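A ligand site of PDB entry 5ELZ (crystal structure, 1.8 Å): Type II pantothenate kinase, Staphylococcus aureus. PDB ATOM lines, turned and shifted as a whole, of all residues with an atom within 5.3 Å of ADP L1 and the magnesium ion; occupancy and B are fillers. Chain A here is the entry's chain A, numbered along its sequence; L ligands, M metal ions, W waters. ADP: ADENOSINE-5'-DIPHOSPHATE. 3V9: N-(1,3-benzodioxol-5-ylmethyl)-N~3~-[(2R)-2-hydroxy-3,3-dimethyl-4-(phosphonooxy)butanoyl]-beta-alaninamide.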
ATOM      1  N   ASP A   6      18.386 -11.386  -7.699  1.00  0.00           N
ATOM      2  CA  ASP A   6      19.663 -11.640  -8.329  1.00  0.00           C
ATOM      3  C   ASP A   6      19.495 -11.343  -9.816  1.00  0.00           C
ATOM      4  O   ASP A   6      18.918 -12.139 -10.562  1.00  0.00           O
ATOM      5  CB  ASP A   6      20.096 -13.083  -8.082  1.00  0.00           C
ATOM      6  CG  ASP A   6      21.426 -13.424  -8.686  1.00  0.00           C
ATOM      7  OD1 ASP A   6      21.993 -12.602  -9.443  1.00  0.00           O
ATOM      8  OD2 ASP A   6      21.919 -14.537  -8.419  1.00  0.00           O
ATOM      9  N   GLY A   8      21.016 -11.224 -12.980  1.00  0.00           N
ATOM     10  CA  GLY A   8      22.194 -11.728 -13.654  1.00  0.00           C
ATOM     11  C   GLY A   8      22.282 -11.320 -15.107  1.00  0.00           C
ATOM     12  O   GLY A   8      21.493 -10.524 -15.589  1.00  0.00           O
ATOM     13  N   GLY A   9      23.263 -11.892 -15.799  1.00  0.00           N
ATOM     14  CA  GLY A   9      23.485 -11.618 -17.222  1.00  0.00           C
ATOM     15  C   GLY A   9      22.350 -12.034 -18.152  1.00  0.00           C
ATOM     16  O   GLY A   9      22.145 -11.424 -19.185  1.00  0.00           O
ATOM     17  N   THR A  10      21.607 -13.084 -17.779  1.00  0.00           N
ATOM     18  CA  THR A  10      20.517 -13.588 -18.631  1.00  0.00           C
ATOM     19  C   THR A  10      19.155 -13.660 -17.922  1.00  0.00           C
ATOM     20  O   THR A  10      18.119 -13.359 -18.544  1.00  0.00           O
ATOM     21  CB  THR A  10      20.851 -14.960 -19.223  1.00  0.00           C
ATOM     22  OG1 THR A  10      22.095 -14.877 -19.918  1.00  0.00           O
ATOM     23  CG2 THR A  10      19.769 -15.420 -20.215  1.00  0.00           C
ATOM     24  N   LEU A  11      19.138 -14.070 -16.655  1.00  0.00           N
ATOM     25  CA  LEU A  11      17.884 -14.141 -15.905  1.00  0.00           C
ATOM     26  C   LEU A  11      17.944 -13.337 -14.640  1.00  0.00           C
ATOM     27  O   LEU A  11      18.995 -13.252 -13.974  1.00  0.00           O
ATOM     28  CB  LEU A  11      17.514 -15.580 -15.531  1.00  0.00           C
ATOM     29  CG  LEU A  11      17.333 -16.559 -16.698  1.00  0.00           C
ATOM     30  CD1 LEU A  11      17.182 -17.979 -16.196  1.00  0.00           C
ATOM     31  CD2 LEU A  11      16.152 -16.181 -17.552  1.00  0.00           C
ATOM     32  N   ILE A  12      16.798 -12.756 -14.329  1.00  0.00           N
ATOM     33  CA  ILE A  12      16.561 -12.108 -13.079  1.00  0.00           C
ATOM     34  C   ILE A  12      15.796 -13.075 -12.185  1.00  0.00           C
ATOM     35  O   ILE A  12      14.670 -13.487 -12.506  1.00  0.00           O
ATOM     36  CB  ILE A  12      15.768 -10.808 -13.290  1.00  0.00           C
ATOM     37  CG1 ILE A  12      16.612  -9.839 -14.150  1.00  0.00           C
ATOM     38  CG2 ILE A  12      15.395 -10.186 -11.948  1.00  0.00           C
ATOM     39  CD1 ILE A  12      15.891  -8.589 -14.565  1.00  0.00           C
ATOM     40  N   LYS A  13      16.410 -13.437 -11.064  1.00  0.00           N
ATOM     41  CA  LYS A  13      15.837 -14.383 -10.119  1.00  0.00           C
ATOM     42  C   LYS A  13      15.274 -13.612  -8.959  1.00  0.00           C
ATOM     43  O   LYS A  13      16.000 -12.811  -8.328  1.00  0.00           O
ATOM     44  CB  LYS A  13      16.883 -15.379  -9.609  1.00  0.00           C
ATOM     45  CG  LYS A  13      17.184 -16.523 -10.564  1.00  0.00           C
ATOM     46  CD  LYS A  13      18.004 -16.101 -11.778  1.00  0.00           C
ATOM     47  CE  LYS A  13      19.375 -15.579 -11.381  1.00  0.00           C
ATOM     48  NZ  LYS A  13      20.265 -15.314 -12.542  1.00  0.00           N
ATOM     49  N   LEU A  28      13.424 -12.539 -17.755  1.00  0.00           N
ATOM     50  CA  LEU A  28      14.611 -12.339 -18.588  1.00  0.00           C
ATOM     51  C   LEU A  28      15.225 -10.996 -18.240  1.00  0.00           C
ATOM     52  O   LEU A  28      14.511 -10.012 -18.010  1.00  0.00           O
ATOM     53  CB  LEU A  28      14.235 -12.359 -20.085  1.00  0.00           C
ATOM     54  CG  LEU A  28      13.490 -13.581 -20.620  1.00  0.00           C
ATOM     55  CD1 LEU A  28      13.217 -13.402 -22.106  1.00  0.00           C
ATOM     56  CD2 LEU A  28      14.245 -14.882 -20.386  1.00  0.00           C
ATOM     57  N   THR A  29      16.545 -10.954 -18.195  1.00  0.00           N
ATOM     58  CA  THR A  29      17.250  -9.698 -17.938  1.00  0.00           C
ATOM     59  C   THR A  29      16.922  -8.666 -19.038  1.00  0.00           C
ATOM     60  O   THR A  29      16.857  -7.461 -18.776  1.00  0.00           O
ATOM     61  CB  THR A  29      18.762  -9.955 -17.839  1.00  0.00           C
ATOM     62  OG1 THR A  29      19.024 -10.811 -16.722  1.00  0.00           O
ATOM     63  CG2 THR A  29      19.534  -8.649 -17.640  1.00  0.00           C
ATOM     64  N   GLU A  70      27.709 -10.771  -5.500  1.00  0.00           N
ATOM     65  CA  GLU A  70      27.070 -12.026  -5.857  1.00  0.00           C
ATOM     66  C   GLU A  70      27.777 -13.259  -5.360  1.00  0.00           C
ATOM     67  O   GLU A  70      27.130 -14.263  -5.134  1.00  0.00           O
ATOM     68  CB  GLU A  70      26.777 -12.141  -7.370  1.00  0.00           C
ATOM     69  CG  GLU A  70      27.996 -12.318  -8.262  1.00  0.00           C
ATOM     70  CD  GLU A  70      27.612 -12.537  -9.710  1.00  0.00           C
ATOM     71  OE1 GLU A  70      27.345 -13.687 -10.092  1.00  0.00           O
ATOM     72  OE2 GLU A  70      27.588 -11.550 -10.471  1.00  0.00           O
ATOM     73  N   ASN A  96      28.995 -22.280 -10.251  1.00  0.00           N
ATOM     74  CA  ASN A  96      27.850 -21.491 -10.586  1.00  0.00           C
ATOM     75  C   ASN A  96      27.811 -21.388 -12.096  1.00  0.00           C
ATOM     76  O   ASN A  96      28.529 -20.566 -12.674  1.00  0.00           O
ATOM     77  CB  ASN A  96      27.971 -20.114  -9.919  1.00  0.00           C
ATOM     78  CG  ASN A  96      26.713 -19.296 -10.015  1.00  0.00           C
ATOM     79  OD1 ASN A  96      25.761 -19.641 -10.717  1.00  0.00           O
ATOM     80  ND2 ASN A  96      26.699 -18.170  -9.287  1.00  0.00           N
ATOM     81  N   VAL A  97      27.001 -22.241 -12.730  1.00  0.00           N
ATOM     82  CA  VAL A  97      26.930 -22.315 -14.186  1.00  0.00           C
ATOM     83  C   VAL A  97      25.810 -21.402 -14.661  1.00  0.00           C
ATOM     84  O   VAL A  97      24.693 -21.846 -14.944  1.00  0.00           O
ATOM     85  CB  VAL A  97      26.747 -23.773 -14.685  1.00  0.00           C
ATOM     86  CG1 VAL A  97      26.913 -23.839 -16.190  1.00  0.00           C
ATOM     87  CG2 VAL A  97      27.747 -24.690 -13.994  1.00  0.00           C
ATOM     88  N   GLY A  98      26.132 -20.107 -14.719  1.00  0.00           N
ATOM     89  CA  GLY A  98      25.219 -19.073 -15.164  1.00  0.00           C
ATOM     90  C   GLY A  98      25.428 -18.766 -16.633  1.00  0.00           C
ATOM     91  O   GLY A  98      25.700 -19.653 -17.428  1.00  0.00           O
ATOM     92  N   THR A  99      25.324 -17.487 -16.987  1.00  0.00           N
ATOM     93  CA  THR A  99      25.610 -17.055 -18.345  1.00  0.00           C
ATOM     94  C   THR A  99      27.027 -17.492 -18.648  1.00  0.00           C
ATOM     95  O   THR A  99      27.314 -17.982 -19.718  1.00  0.00           O
ATOM     96  CB  THR A  99      25.441 -15.531 -18.506  1.00  0.00           C
ATOM     97  OG1 THR A  99      24.108 -15.147 -18.155  1.00  0.00           O
ATOM     98  CG2 THR A  99      25.732 -15.103 -19.951  1.00  0.00           C
ATOM     99  N   GLY A 100      27.908 -17.306 -17.652  1.00  0.00           N
ATOM    100  CA  GLY A 100      29.245 -17.883 -17.631  1.00  0.00           C
ATOM    101  C   GLY A 100      29.421 -18.663 -16.332  1.00  0.00           C
ATOM    102  O   GLY A 100      28.536 -18.663 -15.470  1.00  0.00           O
ATOM    103  N   GLY A 121      25.946 -21.229 -19.743  1.00  0.00           N
ATOM    104  CA  GLY A 121      24.632 -21.138 -20.389  1.00  0.00           C
ATOM    105  C   GLY A 121      24.584 -20.212 -21.581  1.00  0.00           C
ATOM    106  O   GLY A 121      23.795 -20.428 -22.496  1.00  0.00           O
ATOM    107  N   GLY A 122      25.369 -19.144 -21.540  1.00  0.00           N
ATOM    108  CA  GLY A 122      25.426 -18.199 -22.653  1.00  0.00           C
ATOM    109  C   GLY A 122      25.977 -18.826 -23.927  1.00  0.00           C
ATOM    110  O   GLY A 122      25.482 -18.567 -25.005  1.00  0.00           O
ATOM    111  N   ILE A 124      25.876 -22.076 -24.566  1.00  0.00           N
ATOM    112  CA  ILE A 124      24.802 -22.993 -25.010  1.00  0.00           C
ATOM    113  C   ILE A 124      23.799 -22.262 -25.925  1.00  0.00           C
ATOM    114  O   ILE A 124      23.504 -22.717 -27.035  1.00  0.00           O
ATOM    115  CB  ILE A 124      24.110 -23.662 -23.801  1.00  0.00           C
ATOM    116  CG1 ILE A 124      25.098 -24.620 -23.133  1.00  0.00           C
ATOM    117  CG2 ILE A 124      22.879 -24.433 -24.260  1.00  0.00           C
ATOM    118  CD1 ILE A 124      24.578 -25.303 -21.877  1.00  0.00           C
ATOM    119  N   GLN A 125      23.281 -21.135 -25.466  1.00  0.00           N
ATOM    120  CA  GLN A 125      22.330 -20.356 -26.265  1.00  0.00           C
ATOM    121  C   GLN A 125      22.957 -19.780 -27.553  1.00  0.00           C
ATOM    122  O   GLN A 125      22.365 -19.808 -28.622  1.00  0.00           O
ATOM    123  CB  GLN A 125      21.776 -19.206 -25.449  1.00  0.00           C
ATOM    124  CG  GLN A 125      20.891 -19.641 -24.302  1.00  0.00           C
ATOM    125  CD  GLN A 125      20.226 -18.492 -23.608  1.00  0.00           C
ATOM    126  OE1 GLN A 125      20.778 -17.909 -22.651  1.00  0.00           O
ATOM    127  NE2 GLN A 125      19.021 -18.194 -24.008  1.00  0.00           N
ATOM    128  N   TYR A 137      14.780 -20.748 -25.777  1.00  0.00           N
ATOM    129  CA  TYR A 137      15.544 -21.628 -24.877  1.00  0.00           C
ATOM    130  C   TYR A 137      14.912 -23.042 -24.692  1.00  0.00           C
ATOM    131  O   TYR A 137      15.628 -24.047 -24.749  1.00  0.00           O
ATOM    132  CB  TYR A 137      15.715 -20.980 -23.500  1.00  0.00           C
ATOM    133  CG  TYR A 137      16.487 -21.845 -22.544  1.00  0.00           C
ATOM    134  CD1 TYR A 137      17.876 -21.902 -22.590  1.00  0.00           C
ATOM    135  CD2 TYR A 137      15.817 -22.649 -21.603  1.00  0.00           C
ATOM    136  CE1 TYR A 137      18.597 -22.711 -21.713  1.00  0.00           C
ATOM    137  CE2 TYR A 137      16.523 -23.450 -20.715  1.00  0.00           C
ATOM    138  CZ  TYR A 137      17.905 -23.495 -20.780  1.00  0.00           C
ATOM    139  OH  TYR A 137      18.597 -24.280 -19.906  1.00  0.00           O
ATOM    140  N   GLY A 224      23.036 -22.912 -10.857  1.00  0.00           N
ATOM    141  CA  GLY A 224      22.886 -22.093 -12.036  1.00  0.00           C
ATOM    142  C   GLY A 224      21.671 -22.512 -12.847  1.00  0.00           C
ATOM    143  O   GLY A 224      21.293 -23.696 -12.881  1.00  0.00           O
ATOM    144  N   SER A 225      21.087 -21.562 -13.540  1.00  0.00           N
ATOM    145  CA  SER A 225      19.902 -21.859 -14.329  1.00  0.00           C
ATOM    146  C   SER A 225      20.254 -22.638 -15.596  1.00  0.00           C
ATOM    147  O   SER A 225      19.386 -23.155 -16.232  1.00  0.00           O
ATOM    148  CB  SER A 225      19.119 -20.568 -14.653  1.00  0.00           C
ATOM    149  OG  SER A 225      18.952 -19.764 -13.485  1.00  0.00           O
ATOM    150  N   SER A 226      21.541 -22.769 -15.944  1.00  0.00           N
ATOM    151  CA  SER A 226      21.933 -23.532 -17.128  1.00  0.00           C
ATOM    152  C   SER A 226      21.438 -24.983 -17.080  1.00  0.00           C
ATOM    153  O   SER A 226      21.305 -25.625 -18.137  1.00  0.00           O
ATOM    154  CB  SER A 226      23.441 -23.518 -17.309  1.00  0.00           C
ATOM    155  OG  SER A 226      23.924 -22.200 -17.403  1.00  0.00           O
ATOM    156  N   HIS A 228      18.428 -25.886 -15.919  1.00  0.00           N
ATOM    157  CA  HIS A 228      16.984 -25.914 -16.098  1.00  0.00           C
ATOM    158  C   HIS A 228      16.615 -26.387 -17.495  1.00  0.00           C
ATOM    159  O   HIS A 228      17.140 -25.882 -18.506  1.00  0.00           O
ATOM    160  CB  HIS A 228      16.339 -24.538 -15.846  1.00  0.00           C
ATOM    161  CG  HIS A 228      14.854 -24.534 -16.091  1.00  0.00           C
ATOM    162  ND1 HIS A 228      13.957 -25.137 -15.231  1.00  0.00           N
ATOM    163  CD2 HIS A 228      14.115 -24.024 -17.104  1.00  0.00           C
ATOM    164  CE1 HIS A 228      12.740 -24.988 -15.704  1.00  0.00           C
ATOM    165  NE2 HIS A 228      12.800 -24.312 -16.831  1.00  0.00           N
ATOM    166  N   ALA A 255      19.453 -22.310  -8.454  1.00  0.00           N
ATOM    167  CA  ALA A 255      19.593 -21.096  -9.274  1.00  0.00           C
ATOM    168  C   ALA A 255      19.224 -19.820  -8.542  1.00  0.00           C
ATOM    169  O   ALA A 255      19.597 -18.734  -8.979  1.00  0.00           O
ATOM    170  CB  ALA A 255      18.771 -21.205 -10.555  1.00  0.00           C
HETATM  171  PB  ADP L   1      22.835 -15.340 -14.881  1.00  0.00           P
HETATM  172  O1B ADP L   1      21.518 -14.799 -15.405  1.00  0.00           O
HETATM  173  O2B ADP L   1      23.038 -15.124 -13.405  1.00  0.00           O
HETATM  174  O3B ADP L   1      24.006 -14.976 -15.694  1.00  0.00           O
HETATM  175  PA  ADP L   1      21.740 -18.063 -14.637  1.00  0.00           P
HETATM  176  O1A ADP L   1      22.298 -18.904 -13.487  1.00  0.00           O
HETATM  177  O2A ADP L   1      20.373 -17.481 -14.474  1.00  0.00           O
HETATM  178  O3A ADP L   1      22.800 -16.938 -15.112  1.00  0.00           O
HETATM  179  O5' ADP L   1      21.757 -19.038 -15.926  1.00  0.00           O
HETATM  180  C5' ADP L   1      21.518 -18.504 -17.219  1.00  0.00           C
HETATM  181  C4' ADP L   1      21.431 -19.623 -18.215  1.00  0.00           C
HETATM  182  O4' ADP L   1      20.384 -20.515 -17.847  1.00  0.00           O
HETATM  183  C3' ADP L   1      21.091 -19.147 -19.608  1.00  0.00           C
HETATM  184  O3' ADP L   1      22.251 -18.716 -20.298  1.00  0.00           O
HETATM  185  C2' ADP L   1      20.451 -20.379 -20.197  1.00  0.00           C
HETATM  186  O2' ADP L   1      21.423 -21.315 -20.673  1.00  0.00           O
HETATM  187  C1' ADP L   1      19.736 -21.007 -19.015  1.00  0.00           C
HETATM  188  N9  ADP L   1      18.263 -20.754 -18.938  1.00  0.00           N
HETATM  189  C8  ADP L   1      17.441 -21.475 -18.129  1.00  0.00           C
HETATM  190  N7  ADP L   1      16.157 -21.049 -18.262  1.00  0.00           N
HETATM  191  C5  ADP L   1      16.151 -20.068 -19.166  1.00  0.00           C
HETATM  192  C6  ADP L   1      15.120 -19.192 -19.772  1.00  0.00           C
HETATM  193  N6  ADP L   1      13.810 -19.304 -19.419  1.00  0.00           N
HETATM  194  N1  ADP L   1      15.528 -18.299 -20.682  1.00  0.00           N
HETATM  195  C2  ADP L   1      16.803 -18.151 -21.055  1.00  0.00           C
HETATM  196  N3  ADP L   1      17.788 -18.907 -20.534  1.00  0.00           N
HETATM  197  C4  ADP L   1      17.525 -19.875 -19.606  1.00  0.00           C
HETATM  198  O1  3V9 L   2      25.965 -13.352 -14.468  1.00  0.00           O
HETATM  199  O2  3V9 L   2      25.917 -15.104 -12.703  1.00  0.00           O
HETATM  200  O3  3V9 L   2      27.202 -15.524 -14.873  1.00  0.00           O
HETATM  201  P   3V9 L   2      26.586 -14.580 -13.906  1.00  0.00           P
HETATM  202  O01 3V9 L   2      27.941 -13.913 -13.242  1.00  0.00           O
HETATM  203  C02 3V9 L   2      28.852 -13.053 -13.957  1.00  0.00           C
HETATM  204  C03 3V9 L   2      30.315 -13.617 -13.917  1.00  0.00           C
HETATM  205  C04 3V9 L   2      30.874 -13.588 -12.472  1.00  0.00           C
HETATM  206  C25 3V9 L   2      31.208 -12.740 -14.807  1.00  0.00           C
HETATM  207  C05 3V9 L   2      30.336 -15.075 -14.470  1.00  0.00           C
HETATM  208  O24 3V9 L   2      29.662 -15.162 -15.746  1.00  0.00           O
HETATM  209  C06 3V9 L   2      31.771 -15.614 -14.646  1.00  0.00           C
HETATM  210  O23 3V9 L   2      32.484 -15.830 -13.672  1.00  0.00           O
HETATM  211  N07 3V9 L   2      32.168 -15.812 -15.885  1.00  0.00           N
HETATM  212  C08 3V9 L   2      33.498 -16.339 -16.243  1.00  0.00           C
HETATM  213  C09 3V9 L   2      34.591 -15.252 -16.176  1.00  0.00           C
HETATM  214  C10 3V9 L   2      35.954 -15.916 -16.301  1.00  0.00           C
HETATM  215  O22 3V9 L   2      36.507 -16.343 -15.293  1.00  0.00           O
HETATM  216  N11 3V9 L   2      36.463 -16.009 -17.536  1.00  0.00           N
HETATM  217  C12 3V9 L   2      37.707 -16.724 -17.772  1.00  0.00           C
HETATM  218  C13 3V9 L   2      38.500 -16.205 -18.851  1.00  0.00           C
HETATM  219  C21 3V9 L   2      38.482 -14.865 -19.284  1.00  0.00           C
HETATM  220  C17 3V9 L   2      39.298 -14.457 -20.298  1.00  0.00           C
HETATM  221  O18 3V9 L   2      39.418 -13.209 -20.864  1.00  0.00           O
HETATM  222  C19 3V9 L   2      40.350 -13.383 -21.945  1.00  0.00           C
HETATM  223  O20 3V9 L   2      40.902 -14.722 -21.839  1.00  0.00           O
HETATM  224  C16 3V9 L   2      40.163 -15.315 -20.875  1.00  0.00           C
HETATM  225  C15 3V9 L   2      40.227 -16.603 -20.475  1.00  0.00           C
HETATM  226  C14 3V9 L   2      39.407 -17.052 -19.452  1.00  0.00           C
HETATM  227 MG    MG M   1      24.197 -15.501 -11.829  1.00  0.00          MG
HETATM  228  O   HOH W   1      23.994 -13.462 -11.191  1.00  0.00           O
HETATM  229  O   HOH W   2      21.455 -18.321 -10.940  1.00  0.00           O
HETATM  230  O   HOH W   3      14.848 -20.810 -15.653  1.00  0.00           O
HETATM  231  O   HOH W   4      22.579 -15.863 -10.624  1.00  0.00           O
HETATM  232  O   HOH W   5      14.327 -16.780 -22.916  1.00  0.00           O
HETATM  233  O   HOH W   6      17.081 -16.089 -23.818  1.00  0.00           O
HETATM  234  O   HOH W   7      24.409 -17.547 -12.178  1.00  0.00           O
HETATM  235  O   HOH W   8      25.499 -15.735 -10.121  1.00  0.00           O
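N of Gly 122 lies within hydrogen-bond range of O3' of ADP L1 (3.4 Å).
The side-chain amino group of Lys 13 lies within salt-bridge range of an oxygen (O2A) of ADP L1 (2.9 Å).
An oxygen (O3) of 3V9 L2 lies within hydrogen-bond range of the backbone NH (N) of Thr 99 (3.4 Å).
N of Gly 100 sits close to O24 of 3V9 L2, at 3.4 Å.
An oxygen (O2') of ADP L1 lies within hydrogen-bond range of the backbone carbonyl oxygen (O) of Gly 121 (3.1 Å).
OG1 of Thr 99 lies within hydrogen-bond range of O3B of ADP L1 (2.5 Å).
An oxygen (O4') of ADP L1 lies within hydrogen-bond range of the backbone NH of Ser 226, 3.2 Å away.
O1B of ADP L1 sits at hydrogen-bond distance from N of Thr 10, at 2.9 Å.
The backbone NH (N) of Gly 9 sits at hydrogen-bond distance from an oxygen (O1) of 3V9 L2, 3.3 Å away.
The side-chain hydroxyl (OG) of Ser 225 sits at hydrogen-bond distance from an oxygen (O2A) of ADP L1, at 2.9 Å.
The backbone NH of Ser 225 sits at hydrogen-bond distance from an oxygen (O1A) of ADP L1 (2.9 Å).
An oxygen (O3B) of ADP L1 sits at hydrogen-bond distance from the backbone NH of Gly 9, 3.2 Å away.
The side-chain amide oxygen (OE1) of Gln 125 is in hydrogen-bond range of an oxygen (O3') of ADP L1, 2.9 Å away.
An oxygen (O3B) of ADP L1 lies within hydrogen-bond range of the backbone NH (N) of Thr 99, 3.1 Å away.
The backbone NH of Leu 11 is in hydrogen-bond range of an oxygen (O1B) of ADP L1, 2.8 Å away.
The side-chain hydroxyl of Ser 226 is in hydrogen-bond range of the backbone carbonyl oxygen of Val 97 (2.6 Å).
OG of Ser 226 is in hydrogen-bond range of O of Gly 98, 3.1 Å away.
The backbone NH (N) of Gly 122 is in hydrogen-bond range of the backbone carbonyl oxygen (O) of Thr 99, at 2.9 Å.
The backbone carbonyl oxygen (O) of His 228 lies within hydrogen-bond range of the side-chain hydroxyl (OH) of Tyr 137, at 2.6 Å.
The side-chain hydroxyl of Ser 226 lies within hydrogen-bond range of the backbone NH of Gly 121, at 3.2 Å.
The side-chain hydroxyl (OG1) of Thr 29 is in hydrogen-bond range of the backbone carbonyl oxygen (O) of Gly 8 (2.7 Å).
The backbone NH (N) of Gly 121 sits at hydrogen-bond distance from the backbone carbonyl oxygen (O) of Gly 98 (2.8 Å).
The backbone carbonyl oxygen of Leu 11 lies within hydrogen-bond range of the side-chain amino group of Lys 13 (2.8 Å).
Residues that only touch ADP L1: Gly 98, Tyr 137, Gly 8, Gly 224, Leu 28 and His 228.
Hydrophobic or aromatic side chains that line ADP L1: Leu 11, Leu 28, Tyr 137 and His 228.
Within 4 Å of ADP L1: Gly 8, Gly 9, Thr 10, Leu 11, Lys 13, Leu 28, Gly 98, Thr 99, Gly 121, Gly 122, Gln 125, Tyr 137, Gly 224, Ser 225, Ser 226 and His 228.
The nearest printed residue that does not touch ADP L1 is Val 97 (4.1 Å).
No residue comes within 4 Å of the magnesium ion.
The nearest printed residue that does not touch the magnesium ion is Lys 13 (4.0005 Å).
The magnesium ion is bound by an oxygen (O2) of 3V9 L2, an oxygen (O2B) of ADP L1, water W4, water W7, water W1 and water W8.
The magnesium ion has six donor atoms within binding distance.
Water W8 lies within hydrogen-bond range of OE1 of Glu 70 and ND2 of Asn 96.
Water W4 lies within hydrogen-bond range of OD2 of Asp 6 (2.7 Å) and NZ of Lys 13 (3.1 Å).
Water W7 lies within hydrogen-bond range of O1A of ADP L1 (2.8 Å) and OD1 of Asn 96 (2.9 Å).
Water W2 lies within hydrogen-bond range of O of Ala 255 (2.7 Å) and O1A of ADP L1 (2.7 Å).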
